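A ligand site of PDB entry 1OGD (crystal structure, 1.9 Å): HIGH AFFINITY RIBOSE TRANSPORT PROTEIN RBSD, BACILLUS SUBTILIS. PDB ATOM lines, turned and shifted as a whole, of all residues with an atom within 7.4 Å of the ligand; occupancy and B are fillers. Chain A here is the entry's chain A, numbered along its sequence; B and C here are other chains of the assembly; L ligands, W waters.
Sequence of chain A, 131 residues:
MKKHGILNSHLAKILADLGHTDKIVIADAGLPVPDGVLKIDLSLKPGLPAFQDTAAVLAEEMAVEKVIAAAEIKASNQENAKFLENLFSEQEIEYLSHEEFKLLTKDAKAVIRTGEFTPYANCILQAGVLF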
ATOM      1  N   ALA A  27      18.377   9.559   3.009  1.00  0.00           N
ATOM      2  CA  ALA A  27      17.062  10.179   3.124  1.00  0.00           C
ATOM      3  C   ALA A  27      16.105   9.916   1.981  1.00  0.00           C
ATOM      4  O   ALA A  27      16.519   9.546   0.882  1.00  0.00           O
ATOM      5  CB  ALA A  27      17.234  11.687   3.287  1.00  0.00           C
ATOM      6  N   ASP A  28      14.811  10.090   2.269  1.00  0.00           N
ATOM      7  CA  ASP A  28      13.803   9.946   1.236  1.00  0.00           C
ATOM      8  C   ASP A  28      13.797  11.297   0.506  1.00  0.00           C
ATOM      9  O   ASP A  28      14.527  12.207   0.901  1.00  0.00           O
ATOM     10  CB  ASP A  28      12.428   9.598   1.829  1.00  0.00           C
ATOM     11  CG  ASP A  28      11.928  10.613   2.849  1.00  0.00           C
ATOM     12  OD1 ASP A  28      11.397  10.164   3.890  1.00  0.00           O
ATOM     13  OD2 ASP A  28      12.026  11.843   2.618  1.00  0.00           O
ATOM     14  N   ALA A  29      12.992  11.419  -0.538  1.00  0.00           N
ATOM     15  CA  ALA A  29      12.944  12.646  -1.318  1.00  0.00           C
ATOM     16  C   ALA A  29      12.417  13.905  -0.615  1.00  0.00           C
ATOM     17  O   ALA A  29      12.525  15.004  -1.163  1.00  0.00           O
ATOM     18  CB  ALA A  29      12.140  12.404  -2.596  1.00  0.00           C
ATOM     19  N   GLY A  30      11.870  13.745   0.580  1.00  0.00           N
ATOM     20  CA  GLY A  30      11.324  14.909   1.254  1.00  0.00           C
ATOM     21  C   GLY A  30      12.097  15.482   2.427  1.00  0.00           C
ATOM     22  O   GLY A  30      11.840  16.615   2.816  1.00  0.00           O
ATOM     23  N   LEU A  31      13.040  14.737   2.980  1.00  0.00           N
ATOM     24  CA  LEU A  31      13.798  15.223   4.121  1.00  0.00           C
ATOM     25  C   LEU A  31      14.546  16.535   3.857  1.00  0.00           C
ATOM     26  O   LEU A  31      15.289  16.649   2.890  1.00  0.00           O
ATOM     27  CB  LEU A  31      14.800  14.175   4.592  1.00  0.00           C
ATOM     28  CG  LEU A  31      15.458  14.498   5.930  1.00  0.00           C
ATOM     29  CD1 LEU A  31      14.459  14.264   7.042  1.00  0.00           C
ATOM     30  CD2 LEU A  31      16.697  13.631   6.132  1.00  0.00           C
ATOM     31  N   PRO A  32      14.354  17.538   4.724  1.00  0.00           N
ATOM     32  CA  PRO A  32      15.075  18.807   4.520  1.00  0.00           C
ATOM     33  C   PRO A  32      16.526  18.600   4.948  1.00  0.00           C
ATOM     34  O   PRO A  32      16.809  17.832   5.873  1.00  0.00           O
ATOM     35  CB  PRO A  32      14.330  19.769   5.436  1.00  0.00           C
ATOM     36  CG  PRO A  32      13.945  18.879   6.598  1.00  0.00           C
ATOM     37  CD  PRO A  32      13.442  17.628   5.879  1.00  0.00           C
ATOM     38  N   ASN A  77       5.728   3.250   7.948  1.00  0.00           N
ATOM     39  CA  ASN A  77       6.463   2.554   6.910  1.00  0.00           C
ATOM     40  C   ASN A  77       6.994   1.222   7.424  1.00  0.00           C
ATOM     41  O   ASN A  77       8.206   1.015   7.527  1.00  0.00           O
ATOM     42  CB  ASN A  77       7.637   3.425   6.448  1.00  0.00           C
ATOM     43  CG  ASN A  77       7.982   3.220   4.989  1.00  0.00           C
ATOM     44  OD1 ASN A  77       8.100   2.084   4.524  1.00  0.00           O
ATOM     45  ND2 ASN A  77       8.142   4.318   4.260  1.00  0.00           N
ATOM     46  N   HIS A  98      10.737  11.984  15.070  1.00  0.00           N
ATOM     47  CA  HIS A  98      11.224  12.577  13.838  1.00  0.00           C
ATOM     48  C   HIS A  98      11.888  13.936  14.090  1.00  0.00           C
ATOM     49  O   HIS A  98      12.837  14.297  13.415  1.00  0.00           O
ATOM     50  CB  HIS A  98      10.075  12.750  12.846  1.00  0.00           C
ATOM     51  CG  HIS A  98      10.518  13.228  11.494  1.00  0.00           C
ATOM     52  ND1 HIS A  98      11.314  12.459  10.663  1.00  0.00           N
ATOM     53  CD2 HIS A  98      10.296  14.385  10.836  1.00  0.00           C
ATOM     54  CE1 HIS A  98      11.553  13.132   9.547  1.00  0.00           C
ATOM     55  NE2 HIS A  98      10.948  14.302   9.631  1.00  0.00           N
ATOM     56  N   GLU A  99      11.379  14.673  15.076  1.00  0.00           N
ATOM     57  CA  GLU A  99      11.930  15.982  15.397  1.00  0.00           C
ATOM     58  C   GLU A  99      13.351  15.883  15.924  1.00  0.00           C
ATOM     59  O   GLU A  99      14.224  16.643  15.503  1.00  0.00           O
ATOM     60  CB  GLU A  99      11.049  16.703  16.426  1.00  0.00           C
ATOM     61  CG  GLU A  99       9.686  17.105  15.885  1.00  0.00           C
ATOM     62  CD  GLU A  99       9.791  17.933  14.613  1.00  0.00           C
ATOM     63  OE1 GLU A  99      10.452  18.998  14.641  1.00  0.00           O
ATOM     64  OE2 GLU A  99       9.217  17.525  13.580  1.00  0.00           O
ATOM     65  N   PHE A 101      15.302  13.418  15.424  1.00  0.00           N
ATOM     66  CA  PHE A 101      16.045  12.876  14.296  1.00  0.00           C
ATOM     67  C   PHE A 101      16.625  14.000  13.448  1.00  0.00           C
ATOM     68  O   PHE A 101      17.828  14.027  13.155  1.00  0.00           O
ATOM     69  CB  PHE A 101      15.126  12.006  13.435  1.00  0.00           C
ATOM     70  CG  PHE A 101      15.813  11.348  12.271  1.00  0.00           C
ATOM     71  CD1 PHE A 101      16.531  10.172  12.454  1.00  0.00           C
ATOM     72  CD2 PHE A 101      15.738  11.898  10.999  1.00  0.00           C
ATOM     73  CE1 PHE A 101      17.172   9.562  11.382  1.00  0.00           C
ATOM     74  CE2 PHE A 101      16.370  11.290   9.923  1.00  0.00           C
ATOM     75  CZ  PHE A 101      17.098  10.124  10.117  1.00  0.00           C
ATOM     76  N   LYS A 102      15.766  14.936  13.035  1.00  0.00           N
ATOM     77  CA  LYS A 102      16.188  16.063  12.214  1.00  0.00           C
ATOM     78  C   LYS A 102      17.294  16.874  12.878  1.00  0.00           C
ATOM     79  O   LYS A 102      18.191  17.376  12.196  1.00  0.00           O
ATOM     80  CB  LYS A 102      14.996  16.953  11.888  1.00  0.00           C
ATOM     81  CG  LYS A 102      14.286  16.541  10.606  1.00  0.00           C
ATOM     82  CD  LYS A 102      12.782  16.736  10.679  1.00  0.00           C
ATOM     83  CE  LYS A 102      12.385  18.181  10.860  1.00  0.00           C
ATOM     84  NZ  LYS A 102      10.905  18.292  10.946  1.00  0.00           N
ATOM     85  N   GLU A 116      13.207   7.684  -2.889  1.00  0.00           N
ATOM     86  CA  GLU A 116      12.174   7.092  -2.056  1.00  0.00           C
ATOM     87  C   GLU A 116      11.021   8.046  -1.745  1.00  0.00           C
ATOM     88  O   GLU A 116      11.210   9.096  -1.136  1.00  0.00           O
ATOM     89  CB  GLU A 116      12.770   6.603  -0.740  1.00  0.00           C
ATOM     90  CG  GLU A 116      11.838   5.740   0.101  1.00  0.00           C
ATOM     91  CD  GLU A 116      11.493   4.431  -0.583  1.00  0.00           C
ATOM     92  OE1 GLU A 116      12.440   3.708  -0.978  1.00  0.00           O
ATOM     93  OE2 GLU A 116      10.295   4.111  -0.721  1.00  0.00           O
ATOM     94  N   PHE A 117       9.814   7.651  -2.168  1.00  0.00           N
ATOM     95  CA  PHE A 117       8.620   8.442  -1.938  1.00  0.00           C
ATOM     96  C   PHE A 117       7.694   7.851  -0.875  1.00  0.00           C
ATOM     97  O   PHE A 117       6.474   7.853  -1.035  1.00  0.00           O
ATOM     98  CB  PHE A 117       7.825   8.608  -3.245  1.00  0.00           C
ATOM     99  CG  PHE A 117       8.090   9.906  -3.961  1.00  0.00           C
ATOM    100  CD1 PHE A 117       9.396  10.324  -4.226  1.00  0.00           C
ATOM    101  CD2 PHE A 117       7.033  10.700  -4.390  1.00  0.00           C
ATOM    102  CE1 PHE A 117       9.639  11.517  -4.916  1.00  0.00           C
ATOM    103  CE2 PHE A 117       7.266  11.895  -5.083  1.00  0.00           C
ATOM    104  CZ  PHE A 117       8.578  12.301  -5.343  1.00  0.00           C
ATOM    105  N   THR A 118       8.264   7.326   0.204  1.00  0.00           N
ATOM    106  CA  THR A 118       7.445   6.772   1.287  1.00  0.00           C
ATOM    107  C   THR A 118       7.832   7.452   2.602  1.00  0.00           C
ATOM    108  O   THR A 118       8.996   7.790   2.811  1.00  0.00           O
ATOM    109  CB  THR A 118       7.599   5.236   1.433  1.00  0.00           C
ATOM    110  OG1 THR A 118       8.949   4.901   1.784  1.00  0.00           O
ATOM    111  CG2 THR A 118       7.222   4.544   0.136  1.00  0.00           C
ATOM    112  N   PRO A 119       6.854   7.660   3.491  1.00  0.00           N
ATOM    113  CA  PRO A 119       6.997   8.305   4.796  1.00  0.00           C
ATOM    114  C   PRO A 119       8.106   7.785   5.723  1.00  0.00           C
ATOM    115  O   PRO A 119       8.224   6.580   5.970  1.00  0.00           O
ATOM    116  CB  PRO A 119       5.622   8.120   5.436  1.00  0.00           C
ATOM    117  CG  PRO A 119       4.716   8.135   4.252  1.00  0.00           C
ATOM    118  CD  PRO A 119       5.446   7.254   3.272  1.00  0.00           C
ATOM    119  N   TYR A 120       8.890   8.729   6.233  1.00  0.00           N
ATOM    120  CA  TYR A 120       9.974   8.462   7.169  1.00  0.00           C
ATOM    121  C   TYR A 120      11.008   7.407   6.766  1.00  0.00           C
ATOM    122  O   TYR A 120      11.544   6.698   7.619  1.00  0.00           O
ATOM    123  CB  TYR A 120       9.387   8.123   8.541  1.00  0.00           C
ATOM    124  CG  TYR A 120       8.346   9.115   8.995  1.00  0.00           C
ATOM    125  CD1 TYR A 120       7.005   8.965   8.650  1.00  0.00           C
ATOM    126  CD2 TYR A 120       8.713  10.249   9.731  1.00  0.00           C
ATOM    127  CE1 TYR A 120       6.051   9.904   9.016  1.00  0.00           C
ATOM    128  CE2 TYR A 120       7.769  11.198  10.109  1.00  0.00           C
ATOM    129  CZ  TYR A 120       6.442  11.027   9.741  1.00  0.00           C
ATOM    130  OH  TYR A 120       5.509  11.970  10.113  1.00  0.00           O
ATOM    131  N   ALA A 121      11.286   7.318   5.479  1.00  0.00           N
ATOM    132  CA  ALA A 121      12.289   6.379   4.996  1.00  0.00           C
ATOM    133  C   ALA A 121      13.638   7.089   5.077  1.00  0.00           C
ATOM    134  O   ALA A 121      14.230   7.427   4.047  1.00  0.00           O
ATOM    135  CB  ALA A 121      11.991   5.970   3.567  1.00  0.00           C
ATOM    136  N   ASN A 122      14.103   7.337   6.303  1.00  0.00           N
ATOM    137  CA  ASN A 122      15.384   8.005   6.541  1.00  0.00           C
ATOM    138  C   ASN A 122      16.123   7.314   7.681  1.00  0.00           C
ATOM    139  O   ASN A 122      15.503   6.792   8.609  1.00  0.00           O
ATOM    140  CB  ASN A 122      15.212   9.471   6.960  1.00  0.00           C
ATOM    141  CG  ASN A 122      14.223  10.229   6.093  1.00  0.00           C
ATOM    142  OD1 ASN A 122      13.080  10.450   6.489  1.00  0.00           O
ATOM    143  ND2 ASN A 122      14.663  10.631   4.907  1.00  0.00           N
ATOM    144  N   GLY B  19      12.982  20.997   0.782  1.00  0.00           N
ATOM    145  CA  GLY B  19      12.621  19.793   1.505  1.00  0.00           C
ATOM    146  C   GLY B  19      11.446  20.208   2.376  1.00  0.00           C
ATOM    147  O   GLY B  19      11.144  21.390   2.473  1.00  0.00           O
ATOM    148  N   HIS B  20      10.779  19.243   3.014  1.00  0.00           N
ATOM    149  CA  HIS B  20       9.640  19.540   3.869  1.00  0.00           C
ATOM    150  C   HIS B  20       9.949  20.579   4.946  1.00  0.00           C
ATOM    151  O   HIS B  20      10.888  20.427   5.724  1.00  0.00           O
ATOM    152  CB  HIS B  20       9.135  18.262   4.527  1.00  0.00           C
ATOM    153  CG  HIS B  20       7.792  18.394   5.174  1.00  0.00           C
ATOM    154  ND1 HIS B  20       7.346  17.537   6.153  1.00  0.00           N
ATOM    155  CD2 HIS B  20       6.780  19.274   4.950  1.00  0.00           C
ATOM    156  CE1 HIS B  20       6.122  17.884   6.516  1.00  0.00           C
ATOM    157  NE2 HIS B  20       5.752  18.923   5.795  1.00  0.00           N
ATOM    158  N   THR B  21       9.121  21.622   4.979  1.00  0.00           N
ATOM    159  CA  THR B  21       9.202  22.738   5.928  1.00  0.00           C
ATOM    160  C   THR B  21      10.150  23.873   5.563  1.00  0.00           C
ATOM    161  O   THR B  21      10.165  24.899   6.247  1.00  0.00           O
ATOM    162  CB  THR B  21       9.522  22.280   7.389  1.00  0.00           C
ATOM    163  OG1 THR B  21      10.893  21.880   7.505  1.00  0.00           O
ATOM    164  CG2 THR B  21       8.609  21.127   7.793  1.00  0.00           C
ATOM    165  N   GLY B 128       5.659  21.880   1.480  1.00  0.00           N
ATOM    166  CA  GLY B 128       4.985  20.689   1.959  1.00  0.00           C
ATOM    167  C   GLY B 128       5.742  19.484   1.452  1.00  0.00           C
ATOM    168  O   GLY B 128       6.903  19.595   1.054  1.00  0.00           O
ATOM    169  N   VAL B 129       5.105  18.317   1.452  1.00  0.00           N
ATOM    170  CA  VAL B 129       5.762  17.113   0.969  1.00  0.00           C
ATOM    171  C   VAL B 129       4.828  16.421  -0.019  1.00  0.00           C
ATOM    172  O   VAL B 129       3.608  16.485   0.141  1.00  0.00           O
ATOM    173  CB  VAL B 129       6.151  16.187   2.142  1.00  0.00           C
ATOM    174  CG1 VAL B 129       4.896  15.693   2.852  1.00  0.00           C
ATOM    175  CG2 VAL B 129       7.003  15.031   1.637  1.00  0.00           C
ATOM    176  N   LEU B 130       5.389  15.779  -1.030  1.00  0.00           N
ATOM    177  CA  LEU B 130       4.584  15.114  -2.063  1.00  0.00           C
ATOM    178  C   LEU B 130       4.127  13.689  -1.771  1.00  0.00           C
ATOM    179  O   LEU B 130       3.576  13.029  -2.649  1.00  0.00           O
ATOM    180  CB  LEU B 130       5.362  15.122  -3.390  1.00  0.00           C
ATOM    181  CG  LEU B 130       5.699  16.499  -3.945  1.00  0.00           C
ATOM    182  CD1 LEU B 130       6.596  16.361  -5.156  1.00  0.00           C
ATOM    183  CD2 LEU B 130       4.404  17.218  -4.293  1.00  0.00           C
ATOM    184  N   PHE B 131       4.336  13.206  -0.554  1.00  0.00           N
ATOM    185  CA  PHE B 131       3.927  11.861  -0.207  1.00  0.00           C
ATOM    186  C   PHE B 131       3.761  11.707   1.302  1.00  0.00           C
ATOM    187  O   PHE B 131       3.878  12.728   2.008  1.00  0.00           O
ATOM    188  CB  PHE B 131       4.960  10.839  -0.720  1.00  0.00           C
ATOM    189  CG  PHE B 131       6.357  11.110  -0.253  1.00  0.00           C
ATOM    190  CD1 PHE B 131       7.193  11.943  -0.994  1.00  0.00           C
ATOM    191  CD2 PHE B 131       6.821  10.586   0.946  1.00  0.00           C
ATOM    192  CE1 PHE B 131       8.469  12.251  -0.533  1.00  0.00           C
ATOM    193  CE2 PHE B 131       8.106  10.891   1.411  1.00  0.00           C
ATOM    194  CZ  PHE B 131       8.933  11.727   0.666  1.00  0.00           C
ATOM    195  OXT PHE B 131       3.520  10.566   1.756  1.00  0.00           O
ATOM    196  N   MET C   1       7.913  21.298  -1.554  1.00  0.00           N
ATOM    197  CA  MET C   1       8.703  20.569  -2.587  1.00  0.00           C
ATOM    198  C   MET C   1       8.339  21.015  -3.981  1.00  0.00           C
ATOM    199  O   MET C   1       7.241  21.487  -4.232  1.00  0.00           O
ATOM    200  CB  MET C   1       8.460  19.057  -2.474  1.00  0.00           C
ATOM    201  CG  MET C   1       9.176  18.378  -1.322  1.00  0.00           C
ATOM    202  SD  MET C   1       8.877  16.593  -1.314  1.00  0.00           S
ATOM    203  CE  MET C   1       9.587  16.127  -2.905  1.00  0.00           C
HETATM  204  C1  LIG L   1      10.118  14.855   5.682  1.00  0.00           C
HETATM  205  C2  LIG L   1      10.492  13.450   5.262  1.00  0.00           C
HETATM  206  C3  LIG L   1       9.743  12.452   6.127  1.00  0.00           C
HETATM  207  C4  LIG L   1       8.225  12.650   6.129  1.00  0.00           C
HETATM  208  C5  LIG L   1       7.960  14.091   6.560  1.00  0.00           C
HETATM  209  O1  LIG L   1      10.637  15.176   6.944  1.00  0.00           O
HETATM  210  O2  LIG L   1      10.162  13.308   3.902  1.00  0.00           O
HETATM  211  O3  LIG L   1      10.057  11.142   5.735  1.00  0.00           O
HETATM  212  O4  LIG L   1       7.679  12.455   4.839  1.00  0.00           O
HETATM  213  O5  LIG L   1       8.681  15.045   5.755  1.00  0.00           O
HETATM  214  O   HOH W   1       4.730  12.439   4.992  1.00  0.00           O
HETATM  215  O   HOH W   2       9.862  17.611   8.212  1.00  0.00           O
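The side-chain carboxylate (OD1) of Asp 28 lies within hydrogen-bond range of an oxygen (O3) of the ligand, 2.5 Å away. N of Tyr 120 sits at hydrogen-bond distance from O3 of the ligand (2.7 Å). A ring nitrogen (NE2) of His 98 lies within hydrogen-bond range of an oxygen (O1) of the ligand, 2.8 Å away. An oxygen (O5) of the ligand sits at hydrogen-bond distance from a ring nitrogen (ND1) of His 20 of chain B (2.9 Å). An oxygen (O3) of the ligand is in hydrogen-bond range of the side-chain amide oxygen of Asn 122 (3.2 Å). N of Leu 31 is in hydrogen-bond range of O2 of the ligand.
The side-chain amide nitrogen (ND2) of Asn 122 lies close to the backbone NH (N) of Asp 28 (2.7 Å). The side-chain carboxylate (OD2) of Asp 28 sits at hydrogen-bond distance from the backbone NH (N) of Gly 30 (2.8 Å). The side-chain carboxylate of Asp 28 is in hydrogen-bond range of the backbone NH of Leu 31 (3.1 Å). The backbone carbonyl oxygen (O) of Ala 121 sits at hydrogen-bond distance from the backbone NH (N) of Asp 28. The backbone carbonyl oxygen of Gly 30 sits at hydrogen-bond distance from the backbone NH of His 20 of chain B. The backbone carbonyl oxygen (O) of Pro 119 lies within hydrogen-bond range of the side-chain amide nitrogen (ND2) of Asn 77 (2.8 Å).
C of Gly 30 touches O2 of the ligand (3.3 Å). Pro 32 touches the ligand (CD to O1, 3.9 Å). C of Pro 119 touches O3 of the ligand, at 3.9 Å. Phe 131 of chain B touches the ligand (CE2 to O4, 3.8 Å). Hydrophobic or aromatic side chains that line the ligand: Leu 31, Pro 32, His 98, His 20 of chain B and Phe 131 of chain B.
Water W2 lies within hydrogen-bond range of O1 of the ligand (2.9 Å), NZ of Lys 102 (3.0 Å) and ND1 of His 20 of chain B (3.3 Å). Water W1 bridges an oxygen (O4) of the ligand (3.0 Å) and the chain-end carboxylate (O) of Phe 131 of chain B (3.1 Å).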
